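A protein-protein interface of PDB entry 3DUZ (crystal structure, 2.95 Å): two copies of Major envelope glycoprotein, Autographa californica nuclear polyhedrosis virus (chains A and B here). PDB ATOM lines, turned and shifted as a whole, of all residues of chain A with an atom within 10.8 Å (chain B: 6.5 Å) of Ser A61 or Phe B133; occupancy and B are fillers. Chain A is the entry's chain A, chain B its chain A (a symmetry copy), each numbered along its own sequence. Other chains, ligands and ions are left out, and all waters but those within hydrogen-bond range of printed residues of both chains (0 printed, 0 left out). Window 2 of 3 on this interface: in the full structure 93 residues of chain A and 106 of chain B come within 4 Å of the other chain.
Gly B60 touches Ser A61.
Ser A61 touches Ser B61.
CB of Phe B133 touches O of Ser A61, 3.6 Å away.
CB of Asn B131 touches O of Thr A66, at 3.8 Å.
Tyr A57 touches none of the printed residues of chain B.
Ser A61 touches four residues of chain B.
Of the printed residues of chain B, Pro A64 touches Asn B131.
Printed residues of chain B within 4 Å of Thr A66: Asn B131 (3.8 Å).
Of chain A, only Ser A61 comes within 4 Å of Asn B58.
No residue of chain A comes within 4 Å of Gly B59.
Printed residues of chain A within 4 Å of Ser B61: Ser A61.
Of the printed residues of chain A, Asn B131 touches Pro A64 and Thr A66.
Of chain A, only Ser A61 (3.6 Å) comes within 4 Å of Phe B133.
The nearest residue of chain B that does not touch Ser A61 is Asn B131 (5.2 Å).
The nearest printed residue of chain A that does not touch Asn B131 is Asp A63 (4.4 Å).
Ser A61 touches Asn B58, but with the chains exchanged Asn A58 does not touch Ser B61 (8.2 Å).
Ser A61 touches Gly B60, but with the chains exchanged Gly A60 does not touch Ser B61 (7.1 Å).
Ser A61 touches its own counterpart, Ser B61.
Ser A61 touches Phe B133, but with the chains exchanged Phe A133 does not touch Ser B61 (8.8 Å).
9 positions are printed for both chains.
Of the 6 pairs that touch across the chains among the printed residues, 1 has its exchanged pair printed and touching as well.
Among the printed residues, no Asp or Glu carboxylate lies within 4 Å of a Lys or Arg side-chain nitrogen of the other chain.
The backbone NH (N) of Gly A59 sits at hydrogen-bond distance from the side-chain hydroxyl (OG1) of Thr A66, at 2.9 Å.
The backbone carbonyl oxygen (O) of Gly A60 sits at hydrogen-bond distance from the side-chain hydroxyl (OG1) of Thr A66, at 2.7 Å.
OG1 of Thr A66 is in hydrogen-bond range of O of Asp A63 (3.4 Å).
N of Asn B58 is in hydrogen-bond range of OD1 of Asn B130 (3.1 Å).
The backbone carbonyl oxygen (O) of Gly B60 is in hydrogen-bond range of the side-chain hydroxyl (OG1) of Thr B66 (2.7 Å).
OD1 of Asn B131 is in hydrogen-bond range of NE2 of His B132 (3.5 Å).
The backbone carbonyl oxygen of Ser A61 lies within hydrogen-bond range of the side-chain amide nitrogen of Asn B58.
O of Pro A64 lies within hydrogen-bond range of ND2 of Asn B131 (3.0 Å).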
ATOM      1  N   TYR A  57     -21.086 -25.254   6.787  1.00  0.00           N
ATOM      2  CA  TYR A  57     -22.358 -25.057   7.478  1.00  0.00           C
ATOM      3  C   TYR A  57     -22.133 -24.384   8.822  1.00  0.00           C
ATOM      4  O   TYR A  57     -21.261 -24.794   9.586  1.00  0.00           O
ATOM      5  CB  TYR A  57     -23.106 -26.387   7.676  1.00  0.00           C
ATOM      6  CG  TYR A  57     -24.309 -26.269   8.601  1.00  0.00           C
ATOM      7  CD1 TYR A  57     -25.516 -25.734   8.147  1.00  0.00           C
ATOM      8  CD2 TYR A  57     -24.230 -26.673   9.936  1.00  0.00           C
ATOM      9  CE1 TYR A  57     -26.613 -25.608   9.001  1.00  0.00           C
ATOM     10  CE2 TYR A  57     -25.317 -26.554  10.794  1.00  0.00           C
ATOM     11  CZ  TYR A  57     -26.503 -26.021  10.321  1.00  0.00           C
ATOM     12  OH  TYR A  57     -27.578 -25.908  11.168  1.00  0.00           O
ATOM     13  N   ASN A  58     -22.932 -23.362   9.113  1.00  0.00           N
ATOM     14  CA  ASN A  58     -22.830 -22.647  10.378  1.00  0.00           C
ATOM     15  C   ASN A  58     -24.044 -22.878  11.282  1.00  0.00           C
ATOM     16  O   ASN A  58     -25.115 -22.301  11.065  1.00  0.00           O
ATOM     17  CB  ASN A  58     -22.594 -21.150  10.139  1.00  0.00           C
ATOM     18  CG  ASN A  58     -22.596 -20.333  11.427  1.00  0.00           C
ATOM     19  OD1 ASN A  58     -22.495 -20.875  12.530  1.00  0.00           O
ATOM     20  ND2 ASN A  58     -22.710 -19.017  11.289  1.00  0.00           N
ATOM     21  N   GLY A  59     -23.858 -23.720  12.294  1.00  0.00           N
ATOM     22  CA  GLY A  59     -24.877 -23.951  13.317  1.00  0.00           C
ATOM     23  C   GLY A  59     -24.438 -23.437  14.678  1.00  0.00           C
ATOM     24  O   GLY A  59     -24.967 -23.868  15.711  1.00  0.00           O
ATOM     25  N   GLY A  60     -23.473 -22.514  14.677  1.00  0.00           N
ATOM     26  CA  GLY A  60     -22.904 -21.975  15.912  1.00  0.00           C
ATOM     27  C   GLY A  60     -21.919 -22.931  16.563  1.00  0.00           C
ATOM     28  O   GLY A  60     -21.735 -24.064  16.107  1.00  0.00           O
ATOM     29  N   SER A  61     -21.293 -22.474  17.644  1.00  0.00           N
ATOM     30  CA  SER A  61     -20.277 -23.246  18.362  1.00  0.00           C
ATOM     31  C   SER A  61     -20.827 -24.529  18.990  1.00  0.00           C
ATOM     32  O   SER A  61     -20.071 -25.459  19.278  1.00  0.00           O
ATOM     33  CB  SER A  61     -19.627 -22.385  19.446  1.00  0.00           C
ATOM     34  OG  SER A  61     -19.310 -21.086  18.969  1.00  0.00           O
ATOM     35  N   LEU A  62     -22.139 -24.574  19.201  1.00  0.00           N
ATOM     36  CA  LEU A  62     -22.778 -25.722  19.833  1.00  0.00           C
ATOM     37  C   LEU A  62     -22.802 -26.904  18.889  1.00  0.00           C
ATOM     38  O   LEU A  62     -22.517 -28.028  19.290  1.00  0.00           O
ATOM     39  CB  LEU A  62     -24.207 -25.378  20.282  1.00  0.00           C
ATOM     40  CG  LEU A  62     -24.382 -24.306  21.374  1.00  0.00           C
ATOM     41  CD1 LEU A  62     -25.868 -23.936  21.579  1.00  0.00           C
ATOM     42  CD2 LEU A  62     -23.709 -24.725  22.698  1.00  0.00           C
ATOM     43  N   ASP A  63     -23.126 -26.632  17.627  1.00  0.00           N
ATOM     44  CA  ASP A  63     -23.333 -27.670  16.630  1.00  0.00           C
ATOM     45  C   ASP A  63     -22.002 -28.311  16.241  1.00  0.00           C
ATOM     46  O   ASP A  63     -21.050 -27.596  15.889  1.00  0.00           O
ATOM     47  CB  ASP A  63     -24.025 -27.071  15.397  1.00  0.00           C
ATOM     48  CG  ASP A  63     -24.880 -28.076  14.643  1.00  0.00           C
ATOM     49  OD1 ASP A  63     -24.575 -29.283  14.668  1.00  0.00           O
ATOM     50  OD2 ASP A  63     -25.866 -27.654  14.012  1.00  0.00           O
ATOM     51  N   PRO A  64     -21.916 -29.656  16.343  1.00  0.00           N
ATOM     52  CA  PRO A  64     -20.808 -30.430  15.766  1.00  0.00           C
ATOM     53  C   PRO A  64     -20.775 -30.358  14.241  1.00  0.00           C
ATOM     54  O   PRO A  64     -19.748 -30.665  13.636  1.00  0.00           O
ATOM     55  CB  PRO A  64     -21.113 -31.868  16.204  1.00  0.00           C
ATOM     56  CG  PRO A  64     -22.017 -31.734  17.371  1.00  0.00           C
ATOM     57  CD  PRO A  64     -22.852 -30.529  17.071  1.00  0.00           C
ATOM     58  N   ASN A  65     -21.889 -29.959  13.632  1.00  0.00           N
ATOM     59  CA  ASN A  65     -21.979 -29.825  12.179  1.00  0.00           C
ATOM     60  C   ASN A  65     -21.447 -28.503  11.632  1.00  0.00           C
ATOM     61  O   ASN A  65     -21.399 -28.302  10.412  1.00  0.00           O
ATOM     62  CB  ASN A  65     -23.414 -30.045  11.709  1.00  0.00           C
ATOM     63  CG  ASN A  65     -23.837 -31.491  11.809  1.00  0.00           C
ATOM     64  OD1 ASN A  65     -23.130 -32.385  11.346  1.00  0.00           O
ATOM     65  ND2 ASN A  65     -24.998 -31.730  12.411  1.00  0.00           N
ATOM     66  N   THR A  66     -21.062 -27.607  12.537  1.00  0.00           N
ATOM     67  CA  THR A  66     -20.373 -26.389  12.159  1.00  0.00           C
ATOM     68  C   THR A  66     -18.944 -26.761  11.742  1.00  0.00           C
ATOM     69  O   THR A  66     -18.106 -27.123  12.579  1.00  0.00           O
ATOM     70  CB  THR A  66     -20.394 -25.369  13.307  1.00  0.00           C
ATOM     71  OG1 THR A  66     -21.754 -25.091  13.650  1.00  0.00           O
ATOM     72  CG2 THR A  66     -19.698 -24.064  12.912  1.00  0.00           C
ATOM     73  N   ARG A  67     -18.699 -26.693  10.433  1.00  0.00           N
ATOM     74  CA  ARG A  67     -17.455 -27.161   9.812  1.00  0.00           C
ATOM     75  C   ARG A  67     -17.278 -26.505   8.449  1.00  0.00           C
ATOM     76  O   ARG A  67     -18.241 -25.990   7.878  1.00  0.00           O
ATOM     77  CB  ARG A  67     -17.487 -28.681   9.629  1.00  0.00           C
ATOM     78  CG  ARG A  67     -18.749 -29.178   8.925  1.00  0.00           C
ATOM     79  CD  ARG A  67     -18.587 -30.547   8.304  1.00  0.00           C
ATOM     80  NE  ARG A  67     -18.421 -31.624   9.282  1.00  0.00           N
ATOM     81  CZ  ARG A  67     -19.416 -32.297   9.857  1.00  0.00           C
ATOM     82  NH1 ARG A  67     -20.686 -32.008   9.574  1.00  0.00           N
ATOM     83  NH2 ARG A  67     -19.139 -33.267  10.725  1.00  0.00           N
ATOM     84  N   ASN A 130     -18.448 -18.760   5.851  1.00  0.00           N
ATOM     85  CA  ASN A 130     -19.480 -19.478   6.590  1.00  0.00           C
ATOM     86  C   ASN A 130     -20.274 -18.575   7.538  1.00  0.00           C
ATOM     87  O   ASN A 130     -20.643 -18.980   8.640  1.00  0.00           O
ATOM     88  CB  ASN A 130     -18.862 -20.648   7.354  1.00  0.00           C
ATOM     89  CG  ASN A 130     -19.891 -21.673   7.769  1.00  0.00           C
ATOM     90  OD1 ASN A 130     -21.043 -21.635   7.324  1.00  0.00           O
ATOM     91  ND2 ASN A 130     -19.485 -22.601   8.622  1.00  0.00           N
ATOM     92  N   PHE A 133     -25.682 -17.909   9.444  1.00  0.00           N
ATOM     93  CA  PHE A 133     -26.149 -18.757  10.537  1.00  0.00           C
ATOM     94  C   PHE A 133     -27.355 -19.613  10.145  1.00  0.00           C
ATOM     95  O   PHE A 133     -28.271 -19.144   9.458  1.00  0.00           O
ATOM     96  CB  PHE A 133     -26.460 -17.927  11.792  1.00  0.00           C
ATOM     97  CG  PHE A 133     -26.787 -18.763  13.001  1.00  0.00           C
ATOM     98  CD1 PHE A 133     -25.769 -19.265  13.811  1.00  0.00           C
ATOM     99  CD2 PHE A 133     -28.109 -19.068  13.320  1.00  0.00           C
ATOM    100  CE1 PHE A 133     -26.067 -20.057  14.929  1.00  0.00           C
ATOM    101  CE2 PHE A 133     -28.419 -19.860  14.433  1.00  0.00           C
ATOM    102  CZ  PHE A 133     -27.397 -20.354  15.240  1.00  0.00           C
ATOM    103  N   ALA A 134     -27.327 -20.867  10.604  1.00  0.00           N
ATOM    104  CA  ALA A 134     -28.333 -21.888  10.285  1.00  0.00           C
ATOM    105  C   ALA A 134     -28.384 -22.238   8.794  1.00  0.00           C
ATOM    106  O   ALA A 134     -29.368 -22.806   8.319  1.00  0.00           O
ATOM    107  CB  ALA A 134     -29.714 -21.479  10.801  1.00  0.00           C
ATOM    108  N   TYR B  57      -9.187 -25.538  21.047  1.00  0.00           N
ATOM    109  CA  TYR B  57     -10.191 -25.546  22.107  1.00  0.00           C
ATOM    110  C   TYR B  57     -11.386 -24.693  21.714  1.00  0.00           C
ATOM    111  O   TYR B  57     -11.222 -23.565  21.254  1.00  0.00           O
ATOM    112  CB  TYR B  57      -9.610 -25.049  23.441  1.00  0.00           C
ATOM    113  CG  TYR B  57     -10.668 -24.807  24.508  1.00  0.00           C
ATOM    114  CD1 TYR B  57     -11.225 -25.870  25.223  1.00  0.00           C
ATOM    115  CD2 TYR B  57     -11.127 -23.517  24.784  1.00  0.00           C
ATOM    116  CE1 TYR B  57     -12.210 -25.649  26.187  1.00  0.00           C
ATOM    117  CE2 TYR B  57     -12.106 -23.287  25.744  1.00  0.00           C
ATOM    118  CZ  TYR B  57     -12.643 -24.355  26.440  1.00  0.00           C
ATOM    119  OH  TYR B  57     -13.606 -24.127  27.390  1.00  0.00           O
ATOM    120  N   ASN B  58     -12.587 -25.230  21.910  1.00  0.00           N
ATOM    121  CA  ASN B  58     -13.810 -24.506  21.592  1.00  0.00           C
ATOM    122  C   ASN B  58     -14.607 -24.124  22.842  1.00  0.00           C
ATOM    123  O   ASN B  58     -15.284 -24.964  23.444  1.00  0.00           O
ATOM    124  CB  ASN B  58     -14.675 -25.304  20.607  1.00  0.00           C
ATOM    125  CG  ASN B  58     -16.022 -24.648  20.329  1.00  0.00           C
ATOM    126  OD1 ASN B  58     -16.237 -23.472  20.632  1.00  0.00           O
ATOM    127  ND2 ASN B  58     -16.940 -25.411  19.746  1.00  0.00           N
ATOM    128  N   GLY B  59     -14.520 -22.850  23.216  1.00  0.00           N
ATOM    129  CA  GLY B  59     -15.316 -22.300  24.311  1.00  0.00           C
ATOM    130  C   GLY B  59     -16.328 -21.281  23.817  1.00  0.00           C
ATOM    131  O   GLY B  59     -16.810 -20.447  24.596  1.00  0.00           O
ATOM    132  N   GLY B  60     -16.653 -21.349  22.523  1.00  0.00           N
ATOM    133  CA  GLY B  60     -17.563 -20.394  21.892  1.00  0.00           C
ATOM    134  C   GLY B  60     -16.895 -19.061  21.600  1.00  0.00           C
ATOM    135  O   GLY B  60     -15.737 -18.834  21.970  1.00  0.00           O
ATOM    136  N   SER B  61     -17.635 -18.170  20.946  1.00  0.00           N
ATOM    137  CA  SER B  61     -17.128 -16.858  20.542  1.00  0.00           C
ATOM    138  C   SER B  61     -16.760 -15.962  21.729  1.00  0.00           C
ATOM    139  O   SER B  61     -15.981 -15.018  21.582  1.00  0.00           O
ATOM    140  CB  SER B  61     -18.155 -16.142  19.663  1.00  0.00           C
ATOM    141  OG  SER B  61     -18.707 -17.010  18.683  1.00  0.00           O
ATOM    142  N   THR B  66     -10.831 -19.814  22.816  1.00  0.00           N
ATOM    143  CA  THR B  66     -11.249 -20.426  21.569  1.00  0.00           C
ATOM    144  C   THR B  66     -10.221 -20.057  20.492  1.00  0.00           C
ATOM    145  O   THR B  66     -10.146 -18.904  20.045  1.00  0.00           O
ATOM    146  CB  THR B  66     -12.669 -19.983  21.191  1.00  0.00           C
ATOM    147  OG1 THR B  66     -13.561 -20.342  22.250  1.00  0.00           O
ATOM    148  CG2 THR B  66     -13.137 -20.646  19.893  1.00  0.00           C
ATOM    149  N   TRP B 101     -10.594 -35.934  20.880  1.00  0.00           N
ATOM    150  CA  TRP B 101     -11.077 -34.818  21.682  1.00  0.00           C
ATOM    151  C   TRP B 101     -11.424 -35.245  23.107  1.00  0.00           C
ATOM    152  O   TRP B 101     -11.222 -36.398  23.492  1.00  0.00           O
ATOM    153  CB  TRP B 101     -12.270 -34.148  21.004  1.00  0.00           C
ATOM    154  CG  TRP B 101     -13.451 -35.041  20.891  1.00  0.00           C
ATOM    155  CD1 TRP B 101     -13.650 -36.031  19.969  1.00  0.00           C
ATOM    156  CD2 TRP B 101     -14.606 -35.034  21.729  1.00  0.00           C
ATOM    157  NE1 TRP B 101     -14.859 -36.643  20.184  1.00  0.00           N
ATOM    158  CE2 TRP B 101     -15.469 -36.051  21.258  1.00  0.00           C
ATOM    159  CE3 TRP B 101     -15.002 -34.269  22.835  1.00  0.00           C
ATOM    160  CZ2 TRP B 101     -16.703 -36.321  21.857  1.00  0.00           C
ATOM    161  CZ3 TRP B 101     -16.227 -34.537  23.431  1.00  0.00           C
ATOM    162  CH2 TRP B 101     -17.064 -35.555  22.940  1.00  0.00           C
ATOM    163  N   ASN B 130     -12.415 -28.318  15.401  1.00  0.00           N
ATOM    164  CA  ASN B 130     -12.696 -27.775  16.725  1.00  0.00           C
ATOM    165  C   ASN B 130     -14.192 -27.726  17.046  1.00  0.00           C
ATOM    166  O   ASN B 130     -14.674 -26.790  17.682  1.00  0.00           O
ATOM    167  CB  ASN B 130     -12.070 -26.389  16.868  1.00  0.00           C
ATOM    168  CG  ASN B 130     -11.937 -25.963  18.311  1.00  0.00           C
ATOM    169  OD1 ASN B 130     -12.118 -26.767  19.232  1.00  0.00           O
ATOM    170  ND2 ASN B 130     -11.615 -24.695  18.523  1.00  0.00           N
ATOM    171  N   ASN B 131     -14.918 -28.753  16.620  1.00  0.00           N
ATOM    172  CA  ASN B 131     -16.376 -28.773  16.709  1.00  0.00           C
ATOM    173  C   ASN B 131     -16.922 -29.512  17.937  1.00  0.00           C
ATOM    174  O   ASN B 131     -18.053 -30.029  17.920  1.00  0.00           O
ATOM    175  CB  ASN B 131     -16.944 -29.397  15.440  1.00  0.00           C
ATOM    176  CG  ASN B 131     -16.317 -30.741  15.132  1.00  0.00           C
ATOM    177  OD1 ASN B 131     -15.257 -31.084  15.665  1.00  0.00           O
ATOM    178  ND2 ASN B 131     -16.969 -31.512  14.272  1.00  0.00           N
ATOM    179  N   HIS B 132     -16.113 -29.568  18.995  1.00  0.00           N
ATOM    180  CA  HIS B 132     -16.529 -30.164  20.255  1.00  0.00           C
ATOM    181  C   HIS B 132     -16.544 -29.074  21.315  1.00  0.00           C
ATOM    182  O   HIS B 132     -15.505 -28.737  21.900  1.00  0.00           O
ATOM    183  CB  HIS B 132     -15.603 -31.319  20.642  1.00  0.00           C
ATOM    184  CG  HIS B 132     -15.433 -32.340  19.559  1.00  0.00           C
ATOM    185  ND1 HIS B 132     -16.426 -33.229  19.208  1.00  0.00           N
ATOM    186  CD2 HIS B 132     -14.387 -32.605  18.741  1.00  0.00           C
ATOM    187  CE1 HIS B 132     -15.998 -34.001  18.227  1.00  0.00           C
ATOM    188  NE2 HIS B 132     -14.761 -33.645  17.927  1.00  0.00           N
ATOM    189  N   PHE B 133     -17.733 -28.514  21.536  1.00  0.00           N
ATOM    190  CA  PHE B 133     -17.923 -27.415  22.480  1.00  0.00           C
ATOM    191  C   PHE B 133     -17.505 -27.782  23.904  1.00  0.00           C
ATOM    192  O   PHE B 133     -17.774 -28.894  24.379  1.00  0.00           O
ATOM    193  CB  PHE B 133     -19.373 -26.906  22.457  1.00  0.00           C
ATOM    194  CG  PHE B 133     -19.590 -25.667  23.285  1.00  0.00           C
ATOM    195  CD1 PHE B 133     -19.333 -24.405  22.753  1.00  0.00           C
ATOM    196  CD2 PHE B 133     -20.030 -25.762  24.604  1.00  0.00           C
ATOM    197  CE1 PHE B 133     -19.518 -23.250  23.525  1.00  0.00           C
ATOM    198  CE2 PHE B 133     -20.216 -24.616  25.387  1.00  0.00           C
ATOM    199  CZ  PHE B 133     -19.962 -23.358  24.846  1.00  0.00           C
ATOM    200  N   ALA B 134     -16.852 -26.822  24.563  1.00  0.00           N
ATOM    201  CA  ALA B 134     -16.284 -26.980  25.908  1.00  0.00           C
ATOM    202  C   ALA B 134     -15.176 -28.036  25.975  1.00  0.00           C
ATOM    203  O   ALA B 134     -14.838 -28.521  27.054  1.00  0.00           O
ATOM    204  CB  ALA B 134     -17.380 -27.269  26.937  1.00  0.00           C
ATOM    205  N   HIS B 135     -14.602 -28.382  24.822  1.00  0.00           N
ATOM    206  CA  HIS B 135     -13.522 -29.372  24.773  1.00  0.00           C
ATOM    207  C   HIS B 135     -12.372 -29.005  23.851  1.00  0.00           C
ATOM    208  O   HIS B 135     -12.549 -28.264  22.879  1.00  0.00           O
ATOM    209  CB  HIS B 135     -14.069 -30.728  24.359  1.00  0.00           C
ATOM    210  CG  HIS B 135     -14.879 -31.385  25.420  1.00  0.00           C
ATOM    211  ND1 HIS B 135     -14.311 -31.978  26.525  1.00  0.00           N
ATOM    212  CD2 HIS B 135     -16.216 -31.524  25.558  1.00  0.00           C
ATOM    213  CE1 HIS B 135     -15.264 -32.467  27.295  1.00  0.00           C
ATOM    214  NE2 HIS B 135     -16.430 -32.205  26.732  1.00  0.00           N
